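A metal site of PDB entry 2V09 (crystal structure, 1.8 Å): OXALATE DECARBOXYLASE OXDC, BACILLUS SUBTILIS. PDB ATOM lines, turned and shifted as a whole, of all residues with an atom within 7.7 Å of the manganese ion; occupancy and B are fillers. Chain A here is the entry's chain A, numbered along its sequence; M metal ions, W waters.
Four residues have an atom within 4 Å of the manganese ion: His 95, His 97, Glu 101 and His 140.
O of Glu 101 sits at hydrogen-bond distance from N of Phe 134. NE1 of Trp 132 sits at hydrogen-bond distance from OE2 of Glu 101 (3.0 Å). A ring nitrogen (ND1) of His 97 is in hydrogen-bond range of the backbone carbonyl oxygen (O) of Glu 99 (3.0 Å). A ring nitrogen (ND1) of His 140 lies within hydrogen-bond range of the backbone carbonyl oxygen of Leu 138, 2.8 Å away. O of Glu 93 is in hydrogen-bond range of ND1 of His 95, 2.6 Å away.
The manganese ion is bound by OE1 of Glu 101, NE2 of His 95, NE2 of His 97, NE2 of His 140, water W1 and water W2. The manganese ion has six donor atoms within binding distance.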
ATOM      1  N   MET A  84      -5.094  24.148  23.379  1.00  0.00           N
ATOM      2  CA  MET A  84      -6.286  24.558  22.658  1.00  0.00           C
ATOM      3  C   MET A  84      -7.491  23.653  23.052  1.00  0.00           C
ATOM      4  O   MET A  84      -7.365  22.439  23.210  1.00  0.00           O
ATOM      5  CB  MET A  84      -6.055  24.513  21.113  1.00  0.00           C
ATOM      6  CG  MET A  84      -7.280  24.878  20.284  1.00  0.00           C
ATOM      7  SD  MET A  84      -6.877  25.152  18.556  1.00  0.00           S
ATOM      8  CE  MET A  84      -5.951  26.668  18.709  1.00  0.00           C
ATOM      9  N   ARG A  92     -11.276  24.863  14.272  1.00  0.00           N
ATOM     10  CA  ARG A  92     -10.079  25.685  14.137  1.00  0.00           C
ATOM     11  C   ARG A  92      -9.825  25.831  12.632  1.00  0.00           C
ATOM     12  O   ARG A  92      -9.565  24.856  11.894  1.00  0.00           O
ATOM     13  CB  ARG A  92      -8.891  25.047  14.823  1.00  0.00           C
ATOM     14  CG  ARG A  92      -7.566  25.840  14.627  1.00  0.00           C
ATOM     15  CD  ARG A  92      -7.506  27.165  15.289  1.00  0.00           C
ATOM     16  NE  ARG A  92      -6.201  27.781  15.004  1.00  0.00           N
ATOM     17  CZ  ARG A  92      -5.920  28.620  13.996  1.00  0.00           C
ATOM     18  NH1 ARG A  92      -6.862  29.010  13.145  1.00  0.00           N
ATOM     19  NH2 ARG A  92      -4.658  29.048  13.826  1.00  0.00           N
ATOM     20  N   GLU A  93     -10.018  27.066  12.219  1.00  0.00           N
ATOM     21  CA  GLU A  93     -10.092  27.485  10.825  1.00  0.00           C
ATOM     22  C   GLU A  93      -8.891  26.990  10.020  1.00  0.00           C
ATOM     23  O   GLU A  93      -7.740  27.053  10.475  1.00  0.00           O
ATOM     24  CB  GLU A  93     -10.149  29.013  10.741  1.00  0.00           C
ATOM     25  CG  GLU A  93     -10.060  29.548   9.347  1.00  0.00           C
ATOM     26  CD  GLU A  93     -10.193  31.059   9.156  1.00  0.00           C
ATOM     27  OE1 GLU A  93     -10.272  31.846  10.120  1.00  0.00           O
ATOM     28  OE2 GLU A  93     -10.148  31.441   7.990  1.00  0.00           O
ATOM     29  N   HIS A  95      -5.874  26.747   7.898  1.00  0.00           N
ATOM     30  CA  HIS A  95      -4.708  27.638   8.061  1.00  0.00           C
ATOM     31  C   HIS A  95      -3.399  26.874   7.796  1.00  0.00           C
ATOM     32  O   HIS A  95      -3.377  25.656   7.626  1.00  0.00           O
ATOM     33  CB  HIS A  95      -4.701  28.228   9.515  1.00  0.00           C
ATOM     34  CG  HIS A  95      -4.353  27.216  10.577  1.00  0.00           C
ATOM     35  ND1 HIS A  95      -5.293  26.387  11.166  1.00  0.00           N
ATOM     36  CD2 HIS A  95      -3.162  26.906  11.166  1.00  0.00           C
ATOM     37  CE1 HIS A  95      -4.689  25.577  12.035  1.00  0.00           C
ATOM     38  NE2 HIS A  95      -3.398  25.897  12.078  1.00  0.00           N
ATOM     39  N   TRP A  96      -2.297  27.640   7.751  1.00  0.00           N
ATOM     40  CA  TRP A  96      -0.994  27.082   7.661  1.00  0.00           C
ATOM     41  C   TRP A  96      -0.013  28.003   8.392  1.00  0.00           C
ATOM     42  O   TRP A  96      -0.335  29.134   8.760  1.00  0.00           O
ATOM     43  CB  TRP A  96      -0.585  26.816   6.184  1.00  0.00           C
ATOM     44  CG  TRP A  96      -0.235  28.073   5.405  1.00  0.00           C
ATOM     45  CD1 TRP A  96       1.026  28.530   5.131  1.00  0.00           C
ATOM     46  CD2 TRP A  96      -1.147  29.021   4.801  1.00  0.00           C
ATOM     47  NE1 TRP A  96       0.944  29.662   4.381  1.00  0.00           N
ATOM     48  CE2 TRP A  96      -0.355  29.975   4.149  1.00  0.00           C
ATOM     49  CE3 TRP A  96      -2.541  29.105   4.690  1.00  0.00           C
ATOM     50  CZ2 TRP A  96      -0.909  31.093   3.464  1.00  0.00           C
ATOM     51  CZ3 TRP A  96      -3.095  30.214   4.000  1.00  0.00           C
ATOM     52  CH2 TRP A  96      -2.277  31.177   3.392  1.00  0.00           C
ATOM     53  N   HIS A  97       1.168  27.471   8.640  1.00  0.00           N
ATOM     54  CA  HIS A  97       2.260  28.243   9.217  1.00  0.00           C
ATOM     55  C   HIS A  97       3.644  27.649   8.889  1.00  0.00           C
ATOM     56  O   HIS A  97       3.759  26.492   8.459  1.00  0.00           O
ATOM     57  CB  HIS A  97       2.099  28.380  10.764  1.00  0.00           C
ATOM     58  CG  HIS A  97       1.470  27.190  11.404  1.00  0.00           C
ATOM     59  ND1 HIS A  97       2.056  25.929  11.421  1.00  0.00           N
ATOM     60  CD2 HIS A  97       0.242  27.041  11.974  1.00  0.00           C
ATOM     61  CE1 HIS A  97       1.227  25.075  11.991  1.00  0.00           C
ATOM     62  NE2 HIS A  97       0.107  25.708  12.296  1.00  0.00           N
ATOM     63  N   GLU A  99       6.029  26.796  10.966  1.00  0.00           N
ATOM     64  CA  GLU A  99       6.432  25.735  11.888  1.00  0.00           C
ATOM     65  C   GLU A  99       5.738  24.428  11.578  1.00  0.00           C
ATOM     66  O   GLU A  99       4.582  24.423  11.185  1.00  0.00           O
ATOM     67  CB  GLU A  99       6.047  26.166  13.296  1.00  0.00           C
ATOM     68  CG  GLU A  99       6.788  27.447  13.740  1.00  0.00           C
ATOM     69  CD  GLU A  99       6.068  28.763  13.348  1.00  0.00           C
ATOM     70  OE1 GLU A  99       4.986  28.785  12.749  1.00  0.00           O
ATOM     71  OE2 GLU A  99       6.609  29.828  13.704  1.00  0.00           O
ATOM     72  N   ALA A 100       6.444  23.325  11.769  1.00  0.00           N
ATOM     73  CA  ALA A 100       5.804  22.028  11.858  1.00  0.00           C
ATOM     74  C   ALA A 100       5.016  22.021  13.199  1.00  0.00           C
ATOM     75  O   ALA A 100       5.302  22.770  14.136  1.00  0.00           O
ATOM     76  CB  ALA A 100       6.868  20.865  11.820  1.00  0.00           C
ATOM     77  N   GLU A 101       3.982  21.212  13.250  1.00  0.00           N
ATOM     78  CA  GLU A 101       3.091  21.125  14.391  1.00  0.00           C
ATOM     79  C   GLU A 101       2.910  19.645  14.769  1.00  0.00           C
ATOM     80  O   GLU A 101       2.624  18.792  13.907  1.00  0.00           O
ATOM     81  CB  GLU A 101       1.738  21.707  14.013  1.00  0.00           C
ATOM     82  CG  GLU A 101       0.580  21.399  14.958  1.00  0.00           C
ATOM     83  CD  GLU A 101      -0.685  22.134  14.524  1.00  0.00           C
ATOM     84  OE1 GLU A 101      -0.552  23.271  14.009  1.00  0.00           O
ATOM     85  OE2 GLU A 101      -1.789  21.575  14.650  1.00  0.00           O
ATOM     86  N   TRP A 132      -1.106  13.909  16.165  1.00  0.00           N
ATOM     87  CA  TRP A 132      -0.878  14.276  14.764  1.00  0.00           C
ATOM     88  C   TRP A 132       0.436  15.030  14.627  1.00  0.00           C
ATOM     89  O   TRP A 132       1.015  15.503  15.604  1.00  0.00           O
ATOM     90  CB  TRP A 132      -2.047  15.033  14.128  1.00  0.00           C
ATOM     91  CG  TRP A 132      -2.340  16.416  14.637  1.00  0.00           C
ATOM     92  CD1 TRP A 132      -1.612  17.535  14.390  1.00  0.00           C
ATOM     93  CD2 TRP A 132      -3.493  16.843  15.389  1.00  0.00           C
ATOM     94  NE1 TRP A 132      -2.210  18.622  14.953  1.00  0.00           N
ATOM     95  CE2 TRP A 132      -3.375  18.240  15.576  1.00  0.00           C
ATOM     96  CE3 TRP A 132      -4.604  16.186  15.941  1.00  0.00           C
ATOM     97  CZ2 TRP A 132      -4.311  19.000  16.306  1.00  0.00           C
ATOM     98  CZ3 TRP A 132      -5.558  16.942  16.639  1.00  0.00           C
ATOM     99  CH2 TRP A 132      -5.389  18.342  16.832  1.00  0.00           C
ATOM    100  N   PHE A 134       1.899  17.747  11.424  1.00  0.00           N
ATOM    101  CA  PHE A 134       1.700  18.466  10.174  1.00  0.00           C
ATOM    102  C   PHE A 134       3.057  19.080   9.837  1.00  0.00           C
ATOM    103  O   PHE A 134       3.528  19.973  10.532  1.00  0.00           O
ATOM    104  CB  PHE A 134       0.662  19.541  10.316  1.00  0.00           C
ATOM    105  CG  PHE A 134      -0.721  19.037  10.757  1.00  0.00           C
ATOM    106  CD1 PHE A 134      -1.180  17.777  10.345  1.00  0.00           C
ATOM    107  CD2 PHE A 134      -1.529  19.821  11.546  1.00  0.00           C
ATOM    108  CE1 PHE A 134      -2.437  17.332  10.728  1.00  0.00           C
ATOM    109  CE2 PHE A 134      -2.819  19.384  11.944  1.00  0.00           C
ATOM    110  CZ  PHE A 134      -3.236  18.107  11.536  1.00  0.00           C
ATOM    111  N   LEU A 138       2.169  23.014   5.420  1.00  0.00           N
ATOM    112  CA  LEU A 138       1.061  22.270   4.811  1.00  0.00           C
ATOM    113  C   LEU A 138      -0.214  22.676   5.496  1.00  0.00           C
ATOM    114  O   LEU A 138      -0.254  22.823   6.747  1.00  0.00           O
ATOM    115  CB  LEU A 138       1.291  20.754   4.834  1.00  0.00           C
ATOM    116  CG  LEU A 138       2.464  20.216   3.986  1.00  0.00           C
ATOM    117  CD1 LEU A 138       2.420  18.714   3.971  1.00  0.00           C
ATOM    118  CD2 LEU A 138       2.474  20.833   2.535  1.00  0.00           C
ATOM    119  N   PRO A 139      -1.251  22.941   4.692  1.00  0.00           N
ATOM    120  CA  PRO A 139      -2.430  23.526   5.311  1.00  0.00           C
ATOM    121  C   PRO A 139      -3.349  22.496   5.940  1.00  0.00           C
ATOM    122  O   PRO A 139      -3.505  21.374   5.410  1.00  0.00           O
ATOM    123  CB  PRO A 139      -3.127  24.212   4.148  1.00  0.00           C
ATOM    124  CG  PRO A 139      -2.790  23.331   2.977  1.00  0.00           C
ATOM    125  CD  PRO A 139      -1.368  22.892   3.232  1.00  0.00           C
ATOM    126  N   HIS A 140      -3.950  22.899   7.047  1.00  0.00           N
ATOM    127  CA  HIS A 140      -4.747  21.988   7.839  1.00  0.00           C
ATOM    128  C   HIS A 140      -5.871  22.699   8.644  1.00  0.00           C
ATOM    129  O   HIS A 140      -5.993  23.953   8.720  1.00  0.00           O
ATOM    130  CB  HIS A 140      -3.808  21.173   8.778  1.00  0.00           C
ATOM    131  CG  HIS A 140      -2.911  22.046   9.625  1.00  0.00           C
ATOM    132  ND1 HIS A 140      -1.687  22.509   9.190  1.00  0.00           N
ATOM    133  CD2 HIS A 140      -3.107  22.590  10.856  1.00  0.00           C
ATOM    134  CE1 HIS A 140      -1.164  23.292  10.120  1.00  0.00           C
ATOM    135  NE2 HIS A 140      -1.987  23.318  11.155  1.00  0.00           N
ATOM    136  N   SER A 141      -6.701  21.866   9.264  1.00  0.00           N
ATOM    137  CA  SER A 141      -7.835  22.269  10.081  1.00  0.00           C
ATOM    138  C   SER A 141      -8.072  21.220  11.164  1.00  0.00           C
ATOM    139  O   SER A 141      -7.633  20.055  11.064  1.00  0.00           O
ATOM    140  CB  SER A 141      -9.138  22.412   9.265  1.00  0.00           C
ATOM    141  OG  SER A 141      -9.581  21.148   8.723  1.00  0.00           O
ATOM    142  N   ILE A 142      -8.830  21.629  12.181  1.00  0.00           N
ATOM    143  CA  ILE A 142      -9.248  20.758  13.261  1.00  0.00           C
ATOM    144  C   ILE A 142     -10.726  21.081  13.523  1.00  0.00           C
ATOM    145  O   ILE A 142     -11.102  22.276  13.593  1.00  0.00           O
ATOM    146  CB  ILE A 142      -8.452  20.990  14.562  1.00  0.00           C
ATOM    147  CG1 ILE A 142      -6.936  21.023  14.319  1.00  0.00           C
ATOM    148  CG2 ILE A 142      -8.814  19.914  15.615  1.00  0.00           C
ATOM    149  CD1 ILE A 142      -6.215  21.938  15.302  1.00  0.00           C
ATOM    150  N   LEU A 153      -0.549  21.334  21.606  1.00  0.00           N
ATOM    151  CA  LEU A 153       0.143  21.515  20.342  1.00  0.00           C
ATOM    152  C   LEU A 153       1.570  21.906  20.642  1.00  0.00           C
ATOM    153  O   LEU A 153       1.822  22.730  21.547  1.00  0.00           O
ATOM    154  CB  LEU A 153      -0.508  22.641  19.525  1.00  0.00           C
ATOM    155  CG  LEU A 153      -1.973  22.419  19.098  1.00  0.00           C
ATOM    156  CD1 LEU A 153      -2.541  23.678  18.469  1.00  0.00           C
ATOM    157  CD2 LEU A 153      -2.159  21.173  18.191  1.00  0.00           C
ATOM    158  N   PHE A 155       5.081  23.312  18.546  1.00  0.00           N
ATOM    159  CA  PHE A 155       5.602  23.901  17.309  1.00  0.00           C
ATOM    160  C   PHE A 155       7.102  23.944  17.412  1.00  0.00           C
ATOM    161  O   PHE A 155       7.605  24.306  18.473  1.00  0.00           O
ATOM    162  CB  PHE A 155       5.061  25.316  17.153  1.00  0.00           C
ATOM    163  CG  PHE A 155       3.550  25.361  17.101  1.00  0.00           C
ATOM    164  CD1 PHE A 155       2.877  25.045  15.941  1.00  0.00           C
ATOM    165  CD2 PHE A 155       2.837  25.592  18.264  1.00  0.00           C
ATOM    166  CE1 PHE A 155       1.466  25.035  15.934  1.00  0.00           C
ATOM    167  CE2 PHE A 155       1.463  25.585  18.265  1.00  0.00           C
ATOM    168  CZ  PHE A 155       0.778  25.303  17.106  1.00  0.00           C
ATOM    169  N   PHE A 160       7.479  30.945  17.911  1.00  0.00           N
ATOM    170  CA  PHE A 160       6.107  30.820  17.424  1.00  0.00           C
ATOM    171  C   PHE A 160       5.182  31.892  18.001  1.00  0.00           C
ATOM    172  O   PHE A 160       5.160  32.141  19.222  1.00  0.00           O
ATOM    173  CB  PHE A 160       5.535  29.423  17.767  1.00  0.00           C
ATOM    174  CG  PHE A 160       4.089  29.249  17.419  1.00  0.00           C
ATOM    175  CD1 PHE A 160       3.697  28.791  16.168  1.00  0.00           C
ATOM    176  CD2 PHE A 160       3.122  29.482  18.385  1.00  0.00           C
ATOM    177  CE1 PHE A 160       2.333  28.586  15.886  1.00  0.00           C
ATOM    178  CE2 PHE A 160       1.779  29.309  18.079  1.00  0.00           C
ATOM    179  CZ  PHE A 160       1.403  28.852  16.843  1.00  0.00           C
ATOM    180  N   THR A 165       0.265  33.123  12.121  1.00  0.00           N
ATOM    181  CA  THR A 165      -0.431  31.973  11.471  1.00  0.00           C
ATOM    182  C   THR A 165      -1.332  32.467  10.312  1.00  0.00           C
ATOM    183  O   THR A 165      -2.032  33.462  10.471  1.00  0.00           O
ATOM    184  CB  THR A 165      -1.158  31.017  12.497  1.00  0.00           C
ATOM    185  OG1 THR A 165      -0.180  30.110  13.094  1.00  0.00           O
ATOM    186  CG2 THR A 165      -2.174  30.139  11.822  1.00  0.00           C
ATOM    187  N   GLN A 167      -4.439  32.335   8.027  1.00  0.00           N
ATOM    188  CA  GLN A 167      -5.817  31.873   7.974  1.00  0.00           C
ATOM    189  C   GLN A 167      -6.377  32.056   6.573  1.00  0.00           C
ATOM    190  O   GLN A 167      -6.246  33.117   6.011  1.00  0.00           O
ATOM    191  CB  GLN A 167      -6.695  32.684   8.908  1.00  0.00           C
ATOM    192  CG  GLN A 167      -7.035  32.018  10.213  1.00  0.00           C
ATOM    193  CD  GLN A 167      -5.897  31.959  11.122  1.00  0.00           C
ATOM    194  OE1 GLN A 167      -5.414  30.871  11.423  1.00  0.00           O
ATOM    195  NE2 GLN A 167      -5.438  33.135  11.588  1.00  0.00           N
HETATM  196 MN    MN M   1      -1.771  24.659  12.972  1.00  0.00          MN
HETATM  197  O   HOH W   1      -2.001  26.069  14.838  1.00  0.00           O
HETATM  198  O   HOH W   2      -3.485  23.591  14.238  1.00  0.00           O
